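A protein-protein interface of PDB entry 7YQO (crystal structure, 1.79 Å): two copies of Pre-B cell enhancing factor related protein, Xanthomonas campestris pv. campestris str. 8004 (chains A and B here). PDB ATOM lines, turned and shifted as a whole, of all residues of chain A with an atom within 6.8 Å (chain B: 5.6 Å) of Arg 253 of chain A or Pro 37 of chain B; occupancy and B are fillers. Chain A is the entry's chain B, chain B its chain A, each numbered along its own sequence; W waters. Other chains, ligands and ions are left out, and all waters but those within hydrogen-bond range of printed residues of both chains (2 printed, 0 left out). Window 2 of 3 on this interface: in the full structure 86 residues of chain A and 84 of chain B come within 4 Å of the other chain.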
ATOM      1  N   THR A 245       6.891   0.681   9.783  1.00  0.00           N
ATOM      2  CA  THR A 245       6.812   0.605   8.327  1.00  0.00           C
ATOM      3  C   THR A 245       6.914  -0.838   7.839  1.00  0.00           C
ATOM      4  O   THR A 245       6.274  -1.202   6.844  1.00  0.00           O
ATOM      5  CB  THR A 245       7.905   1.472   7.683  1.00  0.00           C
ATOM      6  OG1 THR A 245       7.996   2.725   8.377  1.00  0.00           O
ATOM      7  CG2 THR A 245       7.592   1.738   6.210  1.00  0.00           C
ATOM      8  N   ILE A 246       7.703  -1.670   8.526  1.00  0.00           N
ATOM      9  CA  ILE A 246       7.736  -3.093   8.201  1.00  0.00           C
ATOM     10  C   ILE A 246       6.388  -3.734   8.502  1.00  0.00           C
ATOM     11  O   ILE A 246       5.877  -4.539   7.715  1.00  0.00           O
ATOM     12  CB  ILE A 246       8.883  -3.781   8.961  1.00  0.00           C
ATOM     13  CG1 ILE A 246      10.219  -3.185   8.498  1.00  0.00           C
ATOM     14  CG2 ILE A 246       8.817  -5.297   8.781  1.00  0.00           C
ATOM     15  CD1 ILE A 246      11.401  -4.098   8.611  1.00  0.00           C
ATOM     16  N   SER A 248       3.682  -2.388   8.135  1.00  0.00           N
ATOM     17  CA  SER A 248       2.722  -1.951   7.128  1.00  0.00           C
ATOM     18  C   SER A 248       2.636  -2.898   5.934  1.00  0.00           C
ATOM     19  O   SER A 248       1.645  -2.845   5.195  1.00  0.00           O
ATOM     20  CB  SER A 248       3.072  -0.545   6.641  1.00  0.00           C
ATOM     21  OG  SER A 248       4.193  -0.584   5.777  1.00  0.00           O
ATOM     22  N   TRP A 249       3.643  -3.753   5.722  1.00  0.00           N
ATOM     23  CA  TRP A 249       3.591  -4.737   4.643  1.00  0.00           C
ATOM     24  C   TRP A 249       2.651  -5.904   4.934  1.00  0.00           C
ATOM     25  O   TRP A 249       2.359  -6.681   4.019  1.00  0.00           O
ATOM     26  CB  TRP A 249       4.988  -5.299   4.361  1.00  0.00           C
ATOM     27  CG  TRP A 249       5.945  -4.336   3.734  1.00  0.00           C
ATOM     28  CD1 TRP A 249       6.362  -3.138   4.248  1.00  0.00           C
ATOM     29  CD2 TRP A 249       6.635  -4.499   2.485  1.00  0.00           C
ATOM     30  NE1 TRP A 249       7.260  -2.546   3.392  1.00  0.00           N
ATOM     31  CE2 TRP A 249       7.445  -3.358   2.303  1.00  0.00           C
ATOM     32  CE3 TRP A 249       6.642  -5.498   1.500  1.00  0.00           C
ATOM     33  CZ2 TRP A 249       8.253  -3.186   1.175  1.00  0.00           C
ATOM     34  CZ3 TRP A 249       7.446  -5.325   0.380  1.00  0.00           C
ATOM     35  CH2 TRP A 249       8.241  -4.176   0.229  1.00  0.00           C
ATOM     36  N   GLY A 250       2.184  -6.051   6.168  1.00  0.00           N
ATOM     37  CA  GLY A 250       1.372  -7.198   6.558  1.00  0.00           C
ATOM     38  C   GLY A 250       2.219  -8.367   7.017  1.00  0.00           C
ATOM     39  O   GLY A 250       3.321  -8.608   6.524  1.00  0.00           O
ATOM     40  N   ARG A 251       1.682  -9.118   7.991  1.00  0.00           N
ATOM     41  CA  ARG A 251       2.452 -10.205   8.597  1.00  0.00           C
ATOM     42  C   ARG A 251       2.842 -11.258   7.567  1.00  0.00           C
ATOM     43  O   ARG A 251       3.934 -11.836   7.642  1.00  0.00           O
ATOM     44  CB  ARG A 251       1.669 -10.849   9.744  1.00  0.00           C
ATOM     45  CG  ARG A 251       2.551 -11.585  10.757  1.00  0.00           C
ATOM     46  CD  ARG A 251       2.585 -13.090  10.475  1.00  0.00           C
ATOM     47  NE  ARG A 251       3.209 -13.852  11.556  1.00  0.00           N
ATOM     48  CZ  ARG A 251       3.364 -15.173  11.551  1.00  0.00           C
ATOM     49  NH1 ARG A 251       2.940 -15.894  10.520  1.00  0.00           N
ATOM     50  NH2 ARG A 251       3.942 -15.780  12.579  1.00  0.00           N
ATOM     51  N   GLU A 252       1.971 -11.516   6.589  1.00  0.00           N
ATOM     52  CA  GLU A 252       2.294 -12.507   5.570  1.00  0.00           C
ATOM     53  C   GLU A 252       3.409 -12.037   4.642  1.00  0.00           C
ATOM     54  O   GLU A 252       3.999 -12.860   3.939  1.00  0.00           O
ATOM     55  CB  GLU A 252       1.037 -12.870   4.776  1.00  0.00           C
ATOM     56  CG  GLU A 252      -0.100 -13.420   5.653  1.00  0.00           C
ATOM     57  CD  GLU A 252      -0.752 -14.677   5.085  1.00  0.00           C
ATOM     58  OE1 GLU A 252      -1.299 -14.610   3.962  1.00  0.00           O
ATOM     59  OE2 GLU A 252      -0.723 -15.728   5.765  1.00  0.00           O
ATOM     60  N   ARG A 253       3.727 -10.743   4.635  1.00  0.00           N
ATOM     61  CA  ARG A 253       4.813 -10.221   3.814  1.00  0.00           C
ATOM     62  C   ARG A 253       5.906  -9.563   4.656  1.00  0.00           C
ATOM     63  O   ARG A 253       6.561  -8.621   4.200  1.00  0.00           O
ATOM     64  CB  ARG A 253       4.278  -9.241   2.769  1.00  0.00           C
ATOM     65  CG  ARG A 253       3.654  -9.909   1.552  1.00  0.00           C
ATOM     66  CD  ARG A 253       3.408  -8.907   0.426  1.00  0.00           C
ATOM     67  NE  ARG A 253       2.813  -7.666   0.909  1.00  0.00           N
ATOM     68  CZ  ARG A 253       2.824  -6.519   0.236  1.00  0.00           C
ATOM     69  NH1 ARG A 253       3.401  -6.458  -0.956  1.00  0.00           N
ATOM     70  NH2 ARG A 253       2.260  -5.432   0.752  1.00  0.00           N
ATOM     71  N   GLU A 254       6.133 -10.050   5.882  1.00  0.00           N
ATOM     72  CA  GLU A 254       7.201  -9.467   6.691  1.00  0.00           C
ATOM     73  C   GLU A 254       8.579  -9.841   6.166  1.00  0.00           C
ATOM     74  O   GLU A 254       9.509  -9.035   6.262  1.00  0.00           O
ATOM     75  CB  GLU A 254       7.081  -9.882   8.158  1.00  0.00           C
ATOM     76  CG  GLU A 254       5.778  -9.487   8.853  1.00  0.00           C
ATOM     77  CD  GLU A 254       5.468  -7.987   8.849  1.00  0.00           C
ATOM     78  OE1 GLU A 254       5.497  -7.336   7.777  1.00  0.00           O
ATOM     79  OE2 GLU A 254       5.169  -7.458   9.942  1.00  0.00           O
ATOM     80  N   VAL A 255       8.745 -11.047   5.618  1.00  0.00           N
ATOM     81  CA  VAL A 255      10.018 -11.388   4.988  1.00  0.00           C
ATOM     82  C   VAL A 255      10.213 -10.567   3.723  1.00  0.00           C
ATOM     83  O   VAL A 255      11.343 -10.202   3.371  1.00  0.00           O
ATOM     84  CB  VAL A 255      10.117 -12.908   4.736  1.00  0.00           C
ATOM     85  CG1 VAL A 255       8.863 -13.428   4.040  1.00  0.00           C
ATOM     86  CG2 VAL A 255      11.382 -13.250   3.945  1.00  0.00           C
ATOM     87  N   ASP A 256       9.114 -10.246   3.043  1.00  0.00           N
ATOM     88  CA  ASP A 256       9.192  -9.337   1.907  1.00  0.00           C
ATOM     89  C   ASP A 256       9.694  -7.960   2.335  1.00  0.00           C
ATOM     90  O   ASP A 256      10.491  -7.328   1.623  1.00  0.00           O
ATOM     91  CB  ASP A 256       7.823  -9.225   1.226  1.00  0.00           C
ATOM     92  CG  ASP A 256       7.453 -10.472   0.421  1.00  0.00           C
ATOM     93  OD1 ASP A 256       8.340 -11.329   0.207  1.00  0.00           O
ATOM     94  OD2 ASP A 256       6.285 -10.587  -0.011  1.00  0.00           O
ATOM     95  N   ALA A 257       9.254  -7.488   3.506  1.00  0.00           N
ATOM     96  CA  ALA A 257       9.616  -6.149   3.969  1.00  0.00           C
ATOM     97  C   ALA A 257      11.114  -6.031   4.231  1.00  0.00           C
ATOM     98  O   ALA A 257      11.757  -5.077   3.781  1.00  0.00           O
ATOM     99  CB  ALA A 257       8.818  -5.796   5.226  1.00  0.00           C
ATOM    100  N   TYR A 258      11.690  -6.992   4.961  1.00  0.00           N
ATOM    101  CA  TYR A 258      13.128  -6.966   5.220  1.00  0.00           C
ATOM    102  C   TYR A 258      13.923  -7.208   3.949  1.00  0.00           C
ATOM    103  O   TYR A 258      15.033  -6.682   3.790  1.00  0.00           O
ATOM    104  CB  TYR A 258      13.498  -8.010   6.274  1.00  0.00           C
ATOM    105  CG  TYR A 258      13.030  -7.667   7.668  1.00  0.00           C
ATOM    106  CD1 TYR A 258      13.793  -6.857   8.497  1.00  0.00           C
ATOM    107  CD2 TYR A 258      11.819  -8.151   8.156  1.00  0.00           C
ATOM    108  CE1 TYR A 258      13.371  -6.547   9.773  1.00  0.00           C
ATOM    109  CE2 TYR A 258      11.385  -7.838   9.431  1.00  0.00           C
ATOM    110  CZ  TYR A 258      12.168  -7.037  10.237  1.00  0.00           C
ATOM    111  OH  TYR A 258      11.746  -6.717  11.509  1.00  0.00           O
ATOM    112  N   ASN A 260      13.093  -6.121   0.931  1.00  0.00           N
ATOM    113  CA  ASN A 260      13.143  -4.801   0.307  1.00  0.00           C
ATOM    114  C   ASN A 260      14.253  -3.945   0.908  1.00  0.00           C
ATOM    115  O   ASN A 260      14.980  -3.259   0.178  1.00  0.00           O
ATOM    116  CB  ASN A 260      11.786  -4.112   0.460  1.00  0.00           C
ATOM    117  CG  ASN A 260      11.784  -2.685  -0.071  1.00  0.00           C
ATOM    118  OD1 ASN A 260      11.959  -2.459  -1.271  1.00  0.00           O
ATOM    119  ND2 ASN A 260      11.584  -1.716   0.823  1.00  0.00           N
ATOM    120  N   GLN B  35      11.066   2.362   2.263  1.00  0.00           N
ATOM    121  CA  GLN B  35      10.694   1.222   3.084  1.00  0.00           C
ATOM    122  C   GLN B  35       9.207   0.894   3.018  1.00  0.00           C
ATOM    123  O   GLN B  35       8.799  -0.153   3.535  1.00  0.00           O
ATOM    124  CB  GLN B  35      11.114   1.484   4.539  1.00  0.00           C
ATOM    125  CG  GLN B  35      12.605   1.805   4.682  1.00  0.00           C
ATOM    126  CD  GLN B  35      13.015   2.073   6.131  1.00  0.00           C
ATOM    127  OE1 GLN B  35      12.292   1.728   7.071  1.00  0.00           O
ATOM    128  NE2 GLN B  35      14.180   2.693   6.313  1.00  0.00           N
ATOM    129  N   TYR B  36       8.388   1.756   2.397  1.00  0.00           N
ATOM    130  CA  TYR B  36       6.953   1.536   2.340  1.00  0.00           C
ATOM    131  C   TYR B  36       6.619   0.457   1.311  1.00  0.00           C
ATOM    132  O   TYR B  36       7.370   0.253   0.355  1.00  0.00           O
ATOM    133  CB  TYR B  36       6.232   2.824   1.966  1.00  0.00           C
ATOM    134  CG  TYR B  36       6.030   3.791   3.107  1.00  0.00           C
ATOM    135  CD1 TYR B  36       4.979   3.642   4.003  1.00  0.00           C
ATOM    136  CD2 TYR B  36       6.887   4.875   3.277  1.00  0.00           C
ATOM    137  CE1 TYR B  36       4.788   4.544   5.045  1.00  0.00           C
ATOM    138  CE2 TYR B  36       6.709   5.774   4.309  1.00  0.00           C
ATOM    139  CZ  TYR B  36       5.661   5.614   5.189  1.00  0.00           C
ATOM    140  OH  TYR B  36       5.504   6.530   6.212  1.00  0.00           O
ATOM    141  N   PRO B  37       5.494  -0.236   1.485  1.00  0.00           N
ATOM    142  CA  PRO B  37       5.094  -1.239   0.495  1.00  0.00           C
ATOM    143  C   PRO B  37       4.931  -0.612  -0.876  1.00  0.00           C
ATOM    144  O   PRO B  37       4.622   0.589  -0.996  1.00  0.00           O
ATOM    145  CB  PRO B  37       3.752  -1.756   1.033  1.00  0.00           C
ATOM    146  CG  PRO B  37       3.632  -1.275   2.427  1.00  0.00           C
ATOM    147  CD  PRO B  37       4.544  -0.115   2.604  1.00  0.00           C
ATOM    148  N   PRO B  38       5.119  -1.392  -1.943  1.00  0.00           N
ATOM    149  CA  PRO B  38       4.791  -0.885  -3.286  1.00  0.00           C
ATOM    150  C   PRO B  38       3.323  -0.492  -3.359  1.00  0.00           C
ATOM    151  O   PRO B  38       2.457  -1.137  -2.763  1.00  0.00           O
ATOM    152  CB  PRO B  38       5.109  -2.069  -4.209  1.00  0.00           C
ATOM    153  CG  PRO B  38       6.006  -2.963  -3.403  1.00  0.00           C
ATOM    154  CD  PRO B  38       5.579  -2.791  -1.975  1.00  0.00           C
ATOM    155  N   GLY B  39       3.054   0.604  -4.057  1.00  0.00           N
ATOM    156  CA  GLY B  39       1.694   1.079  -4.186  1.00  0.00           C
ATOM    157  C   GLY B  39       1.163   1.862  -3.009  1.00  0.00           C
ATOM    158  O   GLY B  39      -0.040   2.135  -2.963  1.00  0.00           O
ATOM    159  N   THR B  40       2.007   2.232  -2.050  1.00  0.00           N
ATOM    160  CA  THR B  40       1.523   3.053  -0.950  1.00  0.00           C
ATOM    161  C   THR B  40       1.207   4.458  -1.444  1.00  0.00           C
ATOM    162  O   THR B  40       1.997   5.069  -2.172  1.00  0.00           O
ATOM    163  CB  THR B  40       2.539   3.104   0.191  1.00  0.00           C
ATOM    164  OG1 THR B  40       2.792   1.778   0.666  1.00  0.00           O
ATOM    165  CG2 THR B  40       1.974   3.921   1.341  1.00  0.00           C
ATOM    166  N   VAL B 399      -2.202   3.101   6.513  1.00  0.00           N
ATOM    167  CA  VAL B 399      -1.659   3.505   5.226  1.00  0.00           C
ATOM    168  C   VAL B 399      -2.678   3.120   4.157  1.00  0.00           C
ATOM    169  O   VAL B 399      -3.522   2.245   4.363  1.00  0.00           O
ATOM    170  CB  VAL B 399      -0.298   2.847   4.925  1.00  0.00           C
ATOM    171  CG1 VAL B 399       0.770   3.302   5.922  1.00  0.00           C
ATOM    172  CG2 VAL B 399      -0.438   1.330   4.942  1.00  0.00           C
ATOM    173  N   VAL B 401      -2.880   1.545   0.460  1.00  0.00           N
ATOM    174  CA  VAL B 401      -2.090   0.724  -0.448  1.00  0.00           C
ATOM    175  C   VAL B 401      -3.030   0.181  -1.517  1.00  0.00           C
ATOM    176  O   VAL B 401      -4.096  -0.357  -1.193  1.00  0.00           O
ATOM    177  CB  VAL B 401      -1.376  -0.428   0.286  1.00  0.00           C
ATOM    178  CG1 VAL B 401      -0.617  -1.301  -0.694  1.00  0.00           C
ATOM    179  CG2 VAL B 401      -0.436   0.116   1.368  1.00  0.00           C
HETATM  180  O   HOH W   1       1.962  -3.919  -1.734  1.00  0.00           O
HETATM  181  O   HOH W   2      11.578  -2.056   3.481  1.00  0.00           O
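Water W2 lies within hydrogen-bond range of ND2 of Asn 260 of chain A (2.7 Å), O of Ala 257 of chain A (3.0 Å) and O of Gln 35 of chain B (3.4 Å).
Water W1 lies within hydrogen-bond range of the guanidinium group (NH2) of Arg 253 of chain A and the backbone carbonyl oxygen (O) of Pro 38 of chain B.
Of the 14 printed residues of chain A, 5 touch a printed residue of chain B.
Hydrophobic or aromatic side chains of chain B within 4 Å of the printed part of chain A: Tyr 36, Pro 37 and Pro 38.
Along chain B the printed residues that touch a printed residue of chain A span positions 35 to 38.
Among the printed residues, 9 pairs touch across the chains.
Among the printed residues, no Asp or Glu carboxylate lies within 4 Å of a Lys or Arg side-chain nitrogen of the other chain.
Thr 245 of chain A touches Gln 35 of chain B (CG2 to O, 3.5 Å).
Thr 245 of chain A touches Tyr 36 of chain B.
Pro 37 of chain B touches Ser 248 of chain A (CD to OG, 3.2 Å).
Tyr 36 of chain B touches Trp 249 of chain A (O to CZ2, 3.6 Å).
Pro 38 of chain B touches Trp 249 of chain A (CD to CH2, 3.7 Å).
Pro 37 of chain B touches Arg 253 of chain A (CB to NH2, 3.98 Å).
Asn 260 of chain A touches Gln 35 of chain B (ND2 to CA, 3.8 Å).
Printed residues of chain B within 4 Å of Ser 248 of chain A: Pro 37 (3.2 Å).
Of chain B, only Pro 37 (3.98 Å) comes within 4 Å of Arg 253 of chain A.
Printed residues of chain B within 4 Å of Asn 260 of chain A: Gln 35 (3.8 Å).
Printed residues of chain A within 4 Å of Gln 35 of chain B: Thr 245, Trp 249 and Asn 260.
Pro 37 of chain B touches three residues of chain A.
The nearest residue of chain A that does not touch Pro 37 of chain B is Thr 245 of chain A (4.7 Å).
No position is printed for both chains.
Of the 9 pairs that touch across the chains among the printed residues, none has its exchanged pair printed and touching as well.
The backbone nitrogen (N) of Pro 37 of chain B sits close to the indole nitrogen (NE1) of Trp 249 of chain A, at 3.5 Å.
The backbone carbonyl oxygen of Gln 35 of chain B is in hydrogen-bond range of the indole nitrogen of Trp 249 of chain A, at 2.8 Å.
O of Pro 37 of chain B lies within hydrogen-bond range of OG1 of Thr 40 of chain B, at 2.7 Å.
The side-chain hydroxyl of Ser 248 of chain A lies within hydrogen-bond range of the backbone carbonyl oxygen of Thr 245 of chain A (2.4 Å).
The backbone carbonyl oxygen of Trp 249 of chain A lies within hydrogen-bond range of the guanidinium group of Arg 253 of chain A (3.3 Å).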
